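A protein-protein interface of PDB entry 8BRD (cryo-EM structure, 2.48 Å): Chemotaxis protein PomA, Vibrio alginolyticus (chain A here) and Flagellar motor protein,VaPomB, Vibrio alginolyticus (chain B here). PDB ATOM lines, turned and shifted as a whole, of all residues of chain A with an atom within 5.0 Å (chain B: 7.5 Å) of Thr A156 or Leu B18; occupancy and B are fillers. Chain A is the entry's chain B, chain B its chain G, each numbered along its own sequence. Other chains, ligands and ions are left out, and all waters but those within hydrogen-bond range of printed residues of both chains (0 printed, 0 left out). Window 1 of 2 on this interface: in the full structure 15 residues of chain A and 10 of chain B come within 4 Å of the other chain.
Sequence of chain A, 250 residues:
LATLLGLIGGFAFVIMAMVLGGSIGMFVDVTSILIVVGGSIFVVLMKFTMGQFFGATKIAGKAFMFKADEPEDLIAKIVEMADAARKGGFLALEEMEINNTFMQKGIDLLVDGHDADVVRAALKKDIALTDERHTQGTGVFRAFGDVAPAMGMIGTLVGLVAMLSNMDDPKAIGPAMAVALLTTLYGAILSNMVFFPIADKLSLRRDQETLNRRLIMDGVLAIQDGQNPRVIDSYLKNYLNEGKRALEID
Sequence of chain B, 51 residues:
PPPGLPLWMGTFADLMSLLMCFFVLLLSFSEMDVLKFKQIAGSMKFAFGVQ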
ATOM      1  N   MET A 151      32.501   9.209  -4.447  1.00  0.00           N
ATOM      2  CA  MET A 151      33.314   8.016  -4.245  1.00  0.00           C
ATOM      3  C   MET A 151      33.090   7.414  -2.868  1.00  0.00           C
ATOM      4  O   MET A 151      33.095   6.187  -2.723  1.00  0.00           O
ATOM      5  CB  MET A 151      34.794   8.343  -4.444  1.00  0.00           C
ATOM      6  CG  MET A 151      35.148   8.856  -5.828  1.00  0.00           C
ATOM      7  SD  MET A 151      34.341   7.999  -7.190  1.00  0.00           S
ATOM      8  CE  MET A 151      34.867   6.314  -6.909  1.00  0.00           C
ATOM      9  N   GLY A 152      32.902   8.254  -1.849  1.00  0.00           N
ATOM     10  CA  GLY A 152      32.567   7.738  -0.533  1.00  0.00           C
ATOM     11  C   GLY A 152      31.269   6.958  -0.529  1.00  0.00           C
ATOM     12  O   GLY A 152      31.166   5.912   0.110  1.00  0.00           O
ATOM     13  N   MET A 153      30.264   7.450  -1.255  1.00  0.00           N
ATOM     14  CA  MET A 153      28.993   6.740  -1.358  1.00  0.00           C
ATOM     15  C   MET A 153      29.125   5.448  -2.153  1.00  0.00           C
ATOM     16  O   MET A 153      28.506   4.442  -1.794  1.00  0.00           O
ATOM     17  CB  MET A 153      27.934   7.645  -1.984  1.00  0.00           C
ATOM     18  CG  MET A 153      26.584   6.973  -2.191  1.00  0.00           C
ATOM     19  SD  MET A 153      25.357   7.448  -0.962  1.00  0.00           S
ATOM     20  CE  MET A 153      25.137   5.904  -0.085  1.00  0.00           C
ATOM     21  N   ILE A 154      29.917   5.453  -3.226  1.00  0.00           N
ATOM     22  CA  ILE A 154      30.178   4.221  -3.968  1.00  0.00           C
ATOM     23  C   ILE A 154      30.837   3.187  -3.060  1.00  0.00           C
ATOM     24  O   ILE A 154      30.472   2.005  -3.062  1.00  0.00           O
ATOM     25  CB  ILE A 154      31.039   4.513  -5.209  1.00  0.00           C
ATOM     26  CG1 ILE A 154      30.187   5.128  -6.319  1.00  0.00           C
ATOM     27  CG2 ILE A 154      31.732   3.245  -5.698  1.00  0.00           C
ATOM     28  CD1 ILE A 154      30.979   5.601  -7.508  1.00  0.00           C
ATOM     29  N   GLY A 155      31.824   3.622  -2.271  1.00  0.00           N
ATOM     30  CA  GLY A 155      32.475   2.712  -1.344  1.00  0.00           C
ATOM     31  C   GLY A 155      31.540   2.211  -0.263  1.00  0.00           C
ATOM     32  O   GLY A 155      31.609   1.050   0.140  1.00  0.00           O
ATOM     33  N   THR A 156      30.651   3.079   0.214  1.00  0.00           N
ATOM     34  CA  THR A 156      29.649   2.664   1.188  1.00  0.00           C
ATOM     35  C   THR A 156      28.722   1.610   0.604  1.00  0.00           C
ATOM     36  O   THR A 156      28.434   0.602   1.249  1.00  0.00           O
ATOM     37  CB  THR A 156      28.850   3.877   1.658  1.00  0.00           C
ATOM     38  OG1 THR A 156      29.623   4.624   2.602  1.00  0.00           O
ATOM     39  CG2 THR A 156      27.542   3.456   2.307  1.00  0.00           C
ATOM     40  N   LEU A 157      28.249   1.827  -0.623  1.00  0.00           N
ATOM     41  CA  LEU A 157      27.355   0.865  -1.260  1.00  0.00           C
ATOM     42  C   LEU A 157      28.048  -0.472  -1.476  1.00  0.00           C
ATOM     43  O   LEU A 157      27.461  -1.529  -1.222  1.00  0.00           O
ATOM     44  CB  LEU A 157      26.841   1.424  -2.585  1.00  0.00           C
ATOM     45  CG  LEU A 157      25.901   2.627  -2.506  1.00  0.00           C
ATOM     46  CD1 LEU A 157      25.966   3.454  -3.777  1.00  0.00           C
ATOM     47  CD2 LEU A 157      24.487   2.172  -2.227  1.00  0.00           C
ATOM     48  N   VAL A 158      29.303  -0.446  -1.928  1.00  0.00           N
ATOM     49  CA  VAL A 158      30.038  -1.689  -2.150  1.00  0.00           C
ATOM     50  C   VAL A 158      30.243  -2.428  -0.834  1.00  0.00           C
ATOM     51  O   VAL A 158      29.994  -3.637  -0.733  1.00  0.00           O
ATOM     52  CB  VAL A 158      31.377  -1.397  -2.848  1.00  0.00           C
ATOM     53  CG1 VAL A 158      32.285  -2.605  -2.783  1.00  0.00           C
ATOM     54  CG2 VAL A 158      31.134  -1.008  -4.274  1.00  0.00           C
ATOM     55  N   GLY A 159      30.682  -1.709   0.200  1.00  0.00           N
ATOM     56  CA  GLY A 159      30.893  -2.339   1.487  1.00  0.00           C
ATOM     57  C   GLY A 159      29.618  -2.852   2.120  1.00  0.00           C
ATOM     58  O   GLY A 159      29.626  -3.891   2.773  1.00  0.00           O
ATOM     59  N   LEU A 160      28.508  -2.142   1.935  1.00  0.00           N
ATOM     60  CA  LEU A 160      27.252  -2.580   2.531  1.00  0.00           C
ATOM     61  C   LEU A 160      26.684  -3.783   1.797  1.00  0.00           C
ATOM     62  O   LEU A 160      26.140  -4.691   2.427  1.00  0.00           O
ATOM     63  CB  LEU A 160      26.249  -1.429   2.556  1.00  0.00           C
ATOM     64  CG  LEU A 160      26.587  -0.301   3.538  1.00  0.00           C
ATOM     65  CD1 LEU A 160      25.472   0.725   3.602  1.00  0.00           C
ATOM     66  CD2 LEU A 160      26.913  -0.849   4.916  1.00  0.00           C
ATOM     67  N   VAL A 161      26.808  -3.824   0.467  1.00  0.00           N
ATOM     68  CA  VAL A 161      26.428  -5.040  -0.244  1.00  0.00           C
ATOM     69  C   VAL A 161      27.273  -6.213   0.234  1.00  0.00           C
ATOM     70  O   VAL A 161      26.742  -7.298   0.513  1.00  0.00           O
ATOM     71  CB  VAL A 161      26.541  -4.842  -1.766  1.00  0.00           C
ATOM     72  CG1 VAL A 161      26.259  -6.151  -2.484  1.00  0.00           C
ATOM     73  CG2 VAL A 161      25.577  -3.773  -2.237  1.00  0.00           C
ATOM     74  N   MET A 177      32.354  -3.384   6.293  1.00  0.00           N
ATOM     75  CA  MET A 177      31.849  -2.194   6.960  1.00  0.00           C
ATOM     76  C   MET A 177      32.950  -1.163   7.162  1.00  0.00           C
ATOM     77  O   MET A 177      32.696   0.042   7.086  1.00  0.00           O
ATOM     78  CB  MET A 177      31.204  -2.570   8.293  1.00  0.00           C
ATOM     79  CG  MET A 177      30.825  -1.372   9.137  1.00  0.00           C
ATOM     80  SD  MET A 177      29.400  -0.507   8.461  1.00  0.00           S
ATOM     81  CE  MET A 177      28.191  -0.847   9.717  1.00  0.00           C
ATOM     82  N   ALA A 180      33.252   0.581   3.877  1.00  0.00           N
ATOM     83  CA  ALA A 180      32.083   1.434   3.682  1.00  0.00           C
ATOM     84  C   ALA A 180      32.172   2.712   4.509  1.00  0.00           C
ATOM     85  O   ALA A 180      31.885   3.806   4.008  1.00  0.00           O
ATOM     86  CB  ALA A 180      30.814   0.661   4.036  1.00  0.00           C
ATOM     87  N   LEU A 181      32.570   2.591   5.775  1.00  0.00           N
ATOM     88  CA  LEU A 181      32.626   3.735   6.674  1.00  0.00           C
ATOM     89  C   LEU A 181      33.808   4.647   6.361  1.00  0.00           C
ATOM     90  O   LEU A 181      33.659   5.872   6.323  1.00  0.00           O
ATOM     91  CB  LEU A 181      32.690   3.245   8.121  1.00  0.00           C
ATOM     92  CG  LEU A 181      32.684   4.275   9.249  1.00  0.00           C
ATOM     93  CD1 LEU A 181      31.467   5.167   9.147  1.00  0.00           C
ATOM     94  CD2 LEU A 181      32.717   3.575  10.591  1.00  0.00           C
ATOM     95  N   THR A 183      35.507   4.993   3.556  1.00  0.00           N
ATOM     96  CA  THR A 183      35.336   5.700   2.292  1.00  0.00           C
ATOM     97  C   THR A 183      34.527   6.975   2.488  1.00  0.00           C
ATOM     98  O   THR A 183      34.876   8.034   1.959  1.00  0.00           O
ATOM     99  CB  THR A 183      34.663   4.787   1.270  1.00  0.00           C
ATOM    100  OG1 THR A 183      33.638   4.030   1.921  1.00  0.00           O
ATOM    101  CG2 THR A 183      35.665   3.845   0.645  1.00  0.00           C
ATOM    102  N   THR A 184      33.435   6.888   3.250  1.00  0.00           N
ATOM    103  CA  THR A 184      32.614   8.059   3.525  1.00  0.00           C
ATOM    104  C   THR A 184      33.360   9.076   4.374  1.00  0.00           C
ATOM    105  O   THR A 184      33.297  10.277   4.093  1.00  0.00           O
ATOM    106  CB  THR A 184      31.314   7.640   4.214  1.00  0.00           C
ATOM    107  OG1 THR A 184      30.499   6.925   3.284  1.00  0.00           O
ATOM    108  CG2 THR A 184      30.539   8.852   4.694  1.00  0.00           C
ATOM    109  N   THR B  11      26.667  13.173   1.758  1.00  0.00           N
ATOM    110  CA  THR B  11      27.281  12.572   2.937  1.00  0.00           C
ATOM    111  C   THR B  11      26.237  12.213   3.985  1.00  0.00           C
ATOM    112  O   THR B  11      26.399  11.229   4.710  1.00  0.00           O
ATOM    113  CB  THR B  11      28.327  13.521   3.532  1.00  0.00           C
ATOM    114  OG1 THR B  11      29.227  13.949   2.506  1.00  0.00           O
ATOM    115  CG2 THR B  11      29.122  12.839   4.635  1.00  0.00           C
ATOM    116  N   PHE B  12      25.161  12.994   4.080  1.00  0.00           N
ATOM    117  CA  PHE B  12      24.107  12.671   5.035  1.00  0.00           C
ATOM    118  C   PHE B  12      23.373  11.398   4.636  1.00  0.00           C
ATOM    119  O   PHE B  12      23.094  10.540   5.481  1.00  0.00           O
ATOM    120  CB  PHE B  12      23.131  13.835   5.173  1.00  0.00           C
ATOM    121  CG  PHE B  12      22.037  13.578   6.163  1.00  0.00           C
ATOM    122  CD1 PHE B  12      22.328  13.446   7.510  1.00  0.00           C
ATOM    123  CD2 PHE B  12      20.725  13.439   5.749  1.00  0.00           C
ATOM    124  CE1 PHE B  12      21.329  13.195   8.426  1.00  0.00           C
ATOM    125  CE2 PHE B  12      19.726  13.188   6.659  1.00  0.00           C
ATOM    126  CZ  PHE B  12      20.028  13.067   8.001  1.00  0.00           C
ATOM    127  N   ALA B  13      23.046  11.266   3.350  1.00  0.00           N
ATOM    128  CA  ALA B  13      22.435  10.033   2.864  1.00  0.00           C
ATOM    129  C   ALA B  13      23.377   8.853   3.055  1.00  0.00           C
ATOM    130  O   ALA B  13      22.951   7.752   3.416  1.00  0.00           O
ATOM    131  CB  ALA B  13      22.040  10.185   1.395  1.00  0.00           C
ATOM    132  N   ASP B  14      24.672   9.078   2.829  1.00  0.00           N
ATOM    133  CA  ASP B  14      25.718   8.105   3.116  1.00  0.00           C
ATOM    134  C   ASP B  14      25.682   7.616   4.557  1.00  0.00           C
ATOM    135  O   ASP B  14      25.672   6.410   4.826  1.00  0.00           O
ATOM    136  CB  ASP B  14      27.068   8.760   2.836  1.00  0.00           C
ATOM    137  CG  ASP B  14      27.944   7.933   1.962  1.00  0.00           C
ATOM    138  OD1 ASP B  14      27.943   6.706   2.123  1.00  0.00           O
ATOM    139  OD2 ASP B  14      28.665   8.521   1.138  1.00  0.00           O
ATOM    140  N   LEU B  15      25.690   8.564   5.495  1.00  0.00           N
ATOM    141  CA  LEU B  15      25.704   8.241   6.917  1.00  0.00           C
ATOM    142  C   LEU B  15      24.439   7.508   7.328  1.00  0.00           C
ATOM    143  O   LEU B  15      24.481   6.556   8.115  1.00  0.00           O
ATOM    144  CB  LEU B  15      25.868   9.528   7.727  1.00  0.00           C
ATOM    145  CG  LEU B  15      25.925   9.415   9.250  1.00  0.00           C
ATOM    146  CD1 LEU B  15      27.103   8.576   9.667  1.00  0.00           C
ATOM    147  CD2 LEU B  15      25.990  10.791   9.873  1.00  0.00           C
ATOM    148  N   MET B  16      23.292   7.956   6.812  1.00  0.00           N
ATOM    149  CA  MET B  16      22.032   7.287   7.099  1.00  0.00           C
ATOM    150  C   MET B  16      22.022   5.861   6.567  1.00  0.00           C
ATOM    151  O   MET B  16      21.541   4.956   7.252  1.00  0.00           O
ATOM    152  CB  MET B  16      20.873   8.089   6.513  1.00  0.00           C
ATOM    153  CG  MET B  16      20.362   9.279   7.335  1.00  0.00           C
ATOM    154  SD  MET B  16      20.351   9.136   9.138  1.00  0.00           S
ATOM    155  CE  MET B  16      21.997   9.673   9.589  1.00  0.00           C
ATOM    156  N   SER B  17      22.552   5.644   5.361  1.00  0.00           N
ATOM    157  CA  SER B  17      22.675   4.295   4.818  1.00  0.00           C
ATOM    158  C   SER B  17      23.570   3.432   5.698  1.00  0.00           C
ATOM    159  O   SER B  17      23.252   2.276   5.990  1.00  0.00           O
ATOM    160  CB  SER B  17      23.231   4.353   3.397  1.00  0.00           C
ATOM    161  OG  SER B  17      22.610   5.368   2.639  1.00  0.00           O
ATOM    162  N   LEU B  18      24.703   3.990   6.126  1.00  0.00           N
ATOM    163  CA  LEU B  18      25.638   3.249   6.966  1.00  0.00           C
ATOM    164  C   LEU B  18      24.989   2.829   8.278  1.00  0.00           C
ATOM    165  O   LEU B  18      25.087   1.670   8.688  1.00  0.00           O
ATOM    166  CB  LEU B  18      26.881   4.099   7.226  1.00  0.00           C
ATOM    167  CG  LEU B  18      27.885   4.206   6.077  1.00  0.00           C
ATOM    168  CD1 LEU B  18      28.883   5.317   6.323  1.00  0.00           C
ATOM    169  CD2 LEU B  18      28.605   2.885   5.918  1.00  0.00           C
ATOM    170  N   LEU B  19      24.305   3.761   8.942  1.00  0.00           N
ATOM    171  CA  LEU B  19      23.675   3.448  10.221  1.00  0.00           C
ATOM    172  C   LEU B  19      22.512   2.481  10.046  1.00  0.00           C
ATOM    173  O   LEU B  19      22.335   1.552  10.842  1.00  0.00           O
ATOM    174  CB  LEU B  19      23.220   4.736  10.900  1.00  0.00           C
ATOM    175  CG  LEU B  19      24.352   5.674  11.324  1.00  0.00           C
ATOM    176  CD1 LEU B  19      23.886   7.113  11.343  1.00  0.00           C
ATOM    177  CD2 LEU B  19      24.891   5.268  12.678  1.00  0.00           C
ATOM    178  N   MET B  20      21.719   2.671   8.993  1.00  0.00           N
ATOM    179  CA  MET B  20      20.626   1.757   8.687  1.00  0.00           C
ATOM    180  C   MET B  20      21.129   0.336   8.478  1.00  0.00           C
ATOM    181  O   MET B  20      20.564  -0.626   9.010  1.00  0.00           O
ATOM    182  CB  MET B  20      19.900   2.252   7.442  1.00  0.00           C
ATOM    183  CG  MET B  20      18.515   1.718   7.269  1.00  0.00           C
ATOM    184  SD  MET B  20      18.154   1.708   5.514  1.00  0.00           S
ATOM    185  CE  MET B  20      19.458   0.633   4.940  1.00  0.00           C
ATOM    186  N   CYS B  21      22.198   0.180   7.698  1.00  0.00           N
ATOM    187  CA  CYS B  21      22.705  -1.157   7.427  1.00  0.00           C
ATOM    188  C   CYS B  21      23.430  -1.734   8.633  1.00  0.00           C
ATOM    189  O   CYS B  21      23.471  -2.956   8.803  1.00  0.00           O
ATOM    190  CB  CYS B  21      23.603  -1.131   6.196  1.00  0.00           C
ATOM    191  SG  CYS B  21      22.674  -1.148   4.653  1.00  0.00           S
ATOM    192  N   PHE B  22      23.976  -0.881   9.500  1.00  0.00           N
ATOM    193  CA  PHE B  22      24.480  -1.365  10.782  1.00  0.00           C
ATOM    194  C   PHE B  22      23.349  -1.923  11.637  1.00  0.00           C
ATOM    195  O   PHE B  22      23.517  -2.939  12.321  1.00  0.00           O
ATOM    196  CB  PHE B  22      25.211  -0.245  11.519  1.00  0.00           C
ATOM    197  CG  PHE B  22      25.879  -0.694  12.785  1.00  0.00           C
ATOM    198  CD1 PHE B  22      26.840  -1.688  12.758  1.00  0.00           C
ATOM    199  CD2 PHE B  22      25.540  -0.134  14.002  1.00  0.00           C
ATOM    200  CE1 PHE B  22      27.451  -2.108  13.914  1.00  0.00           C
ATOM    201  CE2 PHE B  22      26.150  -0.553  15.163  1.00  0.00           C
ATOM    202  CZ  PHE B  22      27.105  -1.540  15.119  1.00  0.00           C
ATOM    203  N   PHE B  23      22.188  -1.270  11.610  1.00  0.00           N
ATOM    204  CA  PHE B  23      21.046  -1.791  12.354  1.00  0.00           C
ATOM    205  C   PHE B  23      20.512  -3.069  11.724  1.00  0.00           C
ATOM    206  O   PHE B  23      20.030  -3.957  12.430  1.00  0.00           O
ATOM    207  CB  PHE B  23      19.951  -0.732  12.456  1.00  0.00           C
ATOM    208  CG  PHE B  23      20.344   0.443  13.288  1.00  0.00           C
ATOM    209  CD1 PHE B  23      20.921   0.260  14.529  1.00  0.00           C
ATOM    210  CD2 PHE B  23      20.153   1.731  12.828  1.00  0.00           C
ATOM    211  CE1 PHE B  23      21.300   1.337  15.293  1.00  0.00           C
ATOM    212  CE2 PHE B  23      20.538   2.810  13.586  1.00  0.00           C
ATOM    213  CZ  PHE B  23      21.108   2.614  14.820  1.00  0.00           C
ATOM    214  N   VAL B  24      20.590  -3.184  10.398  1.00  0.00           N
ATOM    215  CA  VAL B  24      20.247  -4.448   9.746  1.00  0.00           C
ATOM    216  C   VAL B  24      21.202  -5.554  10.182  1.00  0.00           C
ATOM    217  O   VAL B  24      20.781  -6.690  10.441  1.00  0.00           O
ATOM    218  CB  VAL B  24      20.229  -4.287   8.213  1.00  0.00           C
ATOM    219  CG1 VAL B  24      19.860  -5.600   7.548  1.00  0.00           C
ATOM    220  CG2 VAL B  24      19.244  -3.216   7.812  1.00  0.00           C
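C of Gly A152 touches OD2 of Asp B14, 3.5 Å away. CE of Met A153 touches OG of Ser B17, 3.8 Å away. Thr A156 touches Leu B18. Leu A160 touches Ser B17 (CD1 to O, 3.6 Å). CD1 of Leu A160 touches SG of Cys B21, at 3.5 Å. CE of Met A177 touches CD1 of Phe B22 (3.4 Å). Ala A180 touches Leu B18. Leu B18 touches Leu A181. Leu B18 touches Thr A184.
The side-chain hydroxyl (OG1) of Thr A184 is in hydrogen-bond range of the side-chain hydroxyl (OG1) of Thr A156. O of Ala A180 sits at hydrogen-bond distance from OG1 of Thr A184 (3.5 Å). The backbone carbonyl oxygen (O) of Ser B17 sits close to the side-chain sulfur (SG) of Cys B21 (3.7 Å). The side-chain hydroxyl of Thr A183 sits at hydrogen-bond distance from the backbone carbonyl oxygen of Ala A180, at 2.7 Å. OG1 of Thr A184 is in hydrogen-bond range of O of Gly A152, at 3.4 Å. O of Ala B13 sits at hydrogen-bond distance from OG of Ser B17 (2.5 Å).
No residue of chain B comes within 4 Å of Gly A155. Of the printed residues of chain B, Thr A156 touches Asp B14 and Leu B18. Printed residues of chain B within 4 Å of Leu A181: Leu B18 (3.8 Å). Of the printed residues of chain A, Ser B17 touches Met A153 (3.8 Å) and Leu A160 (3.6 Å). Of chain A, only Thr A156, Ala A180, Leu A181 and Thr A184 come within 4 Å of Leu B18. The nearest residue of chain B that does not touch Thr A156 is Ser B17 (4.5 Å). The nearest residue of chain A that does not touch Leu B18 is Met A177 (4.1 Å).
The backbone NH (N) of Met A153 sits at hydrogen-bond distance from the side-chain carboxylate (OD2) of Asp B14, 3.1 Å away. OG1 of Thr A184 sits at hydrogen-bond distance from OD1 of Asp B14 (2.8 Å). OD1 of Asp B14 sits at hydrogen-bond distance from OG1 of Thr A156 (2.7 Å).
Of the 14 printed residues of chain B, 5 touch a printed residue of chain A. Hydrophobic or aromatic side chains of chain B within 4 Å of the printed part of chain A: Leu B18 and Phe B22. Hydrophobic or aromatic side chains of chain A within 4 Å of the printed part of chain B: Met A153, Leu A160, Met A177, Ala A180 and Leu A181. Among the printed residues, 12 pairs touch across the chains. Among the printed residues, no Asp or Glu carboxylate lies within 4 Å of a Lys or Arg side-chain nitrogen of the other chain.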
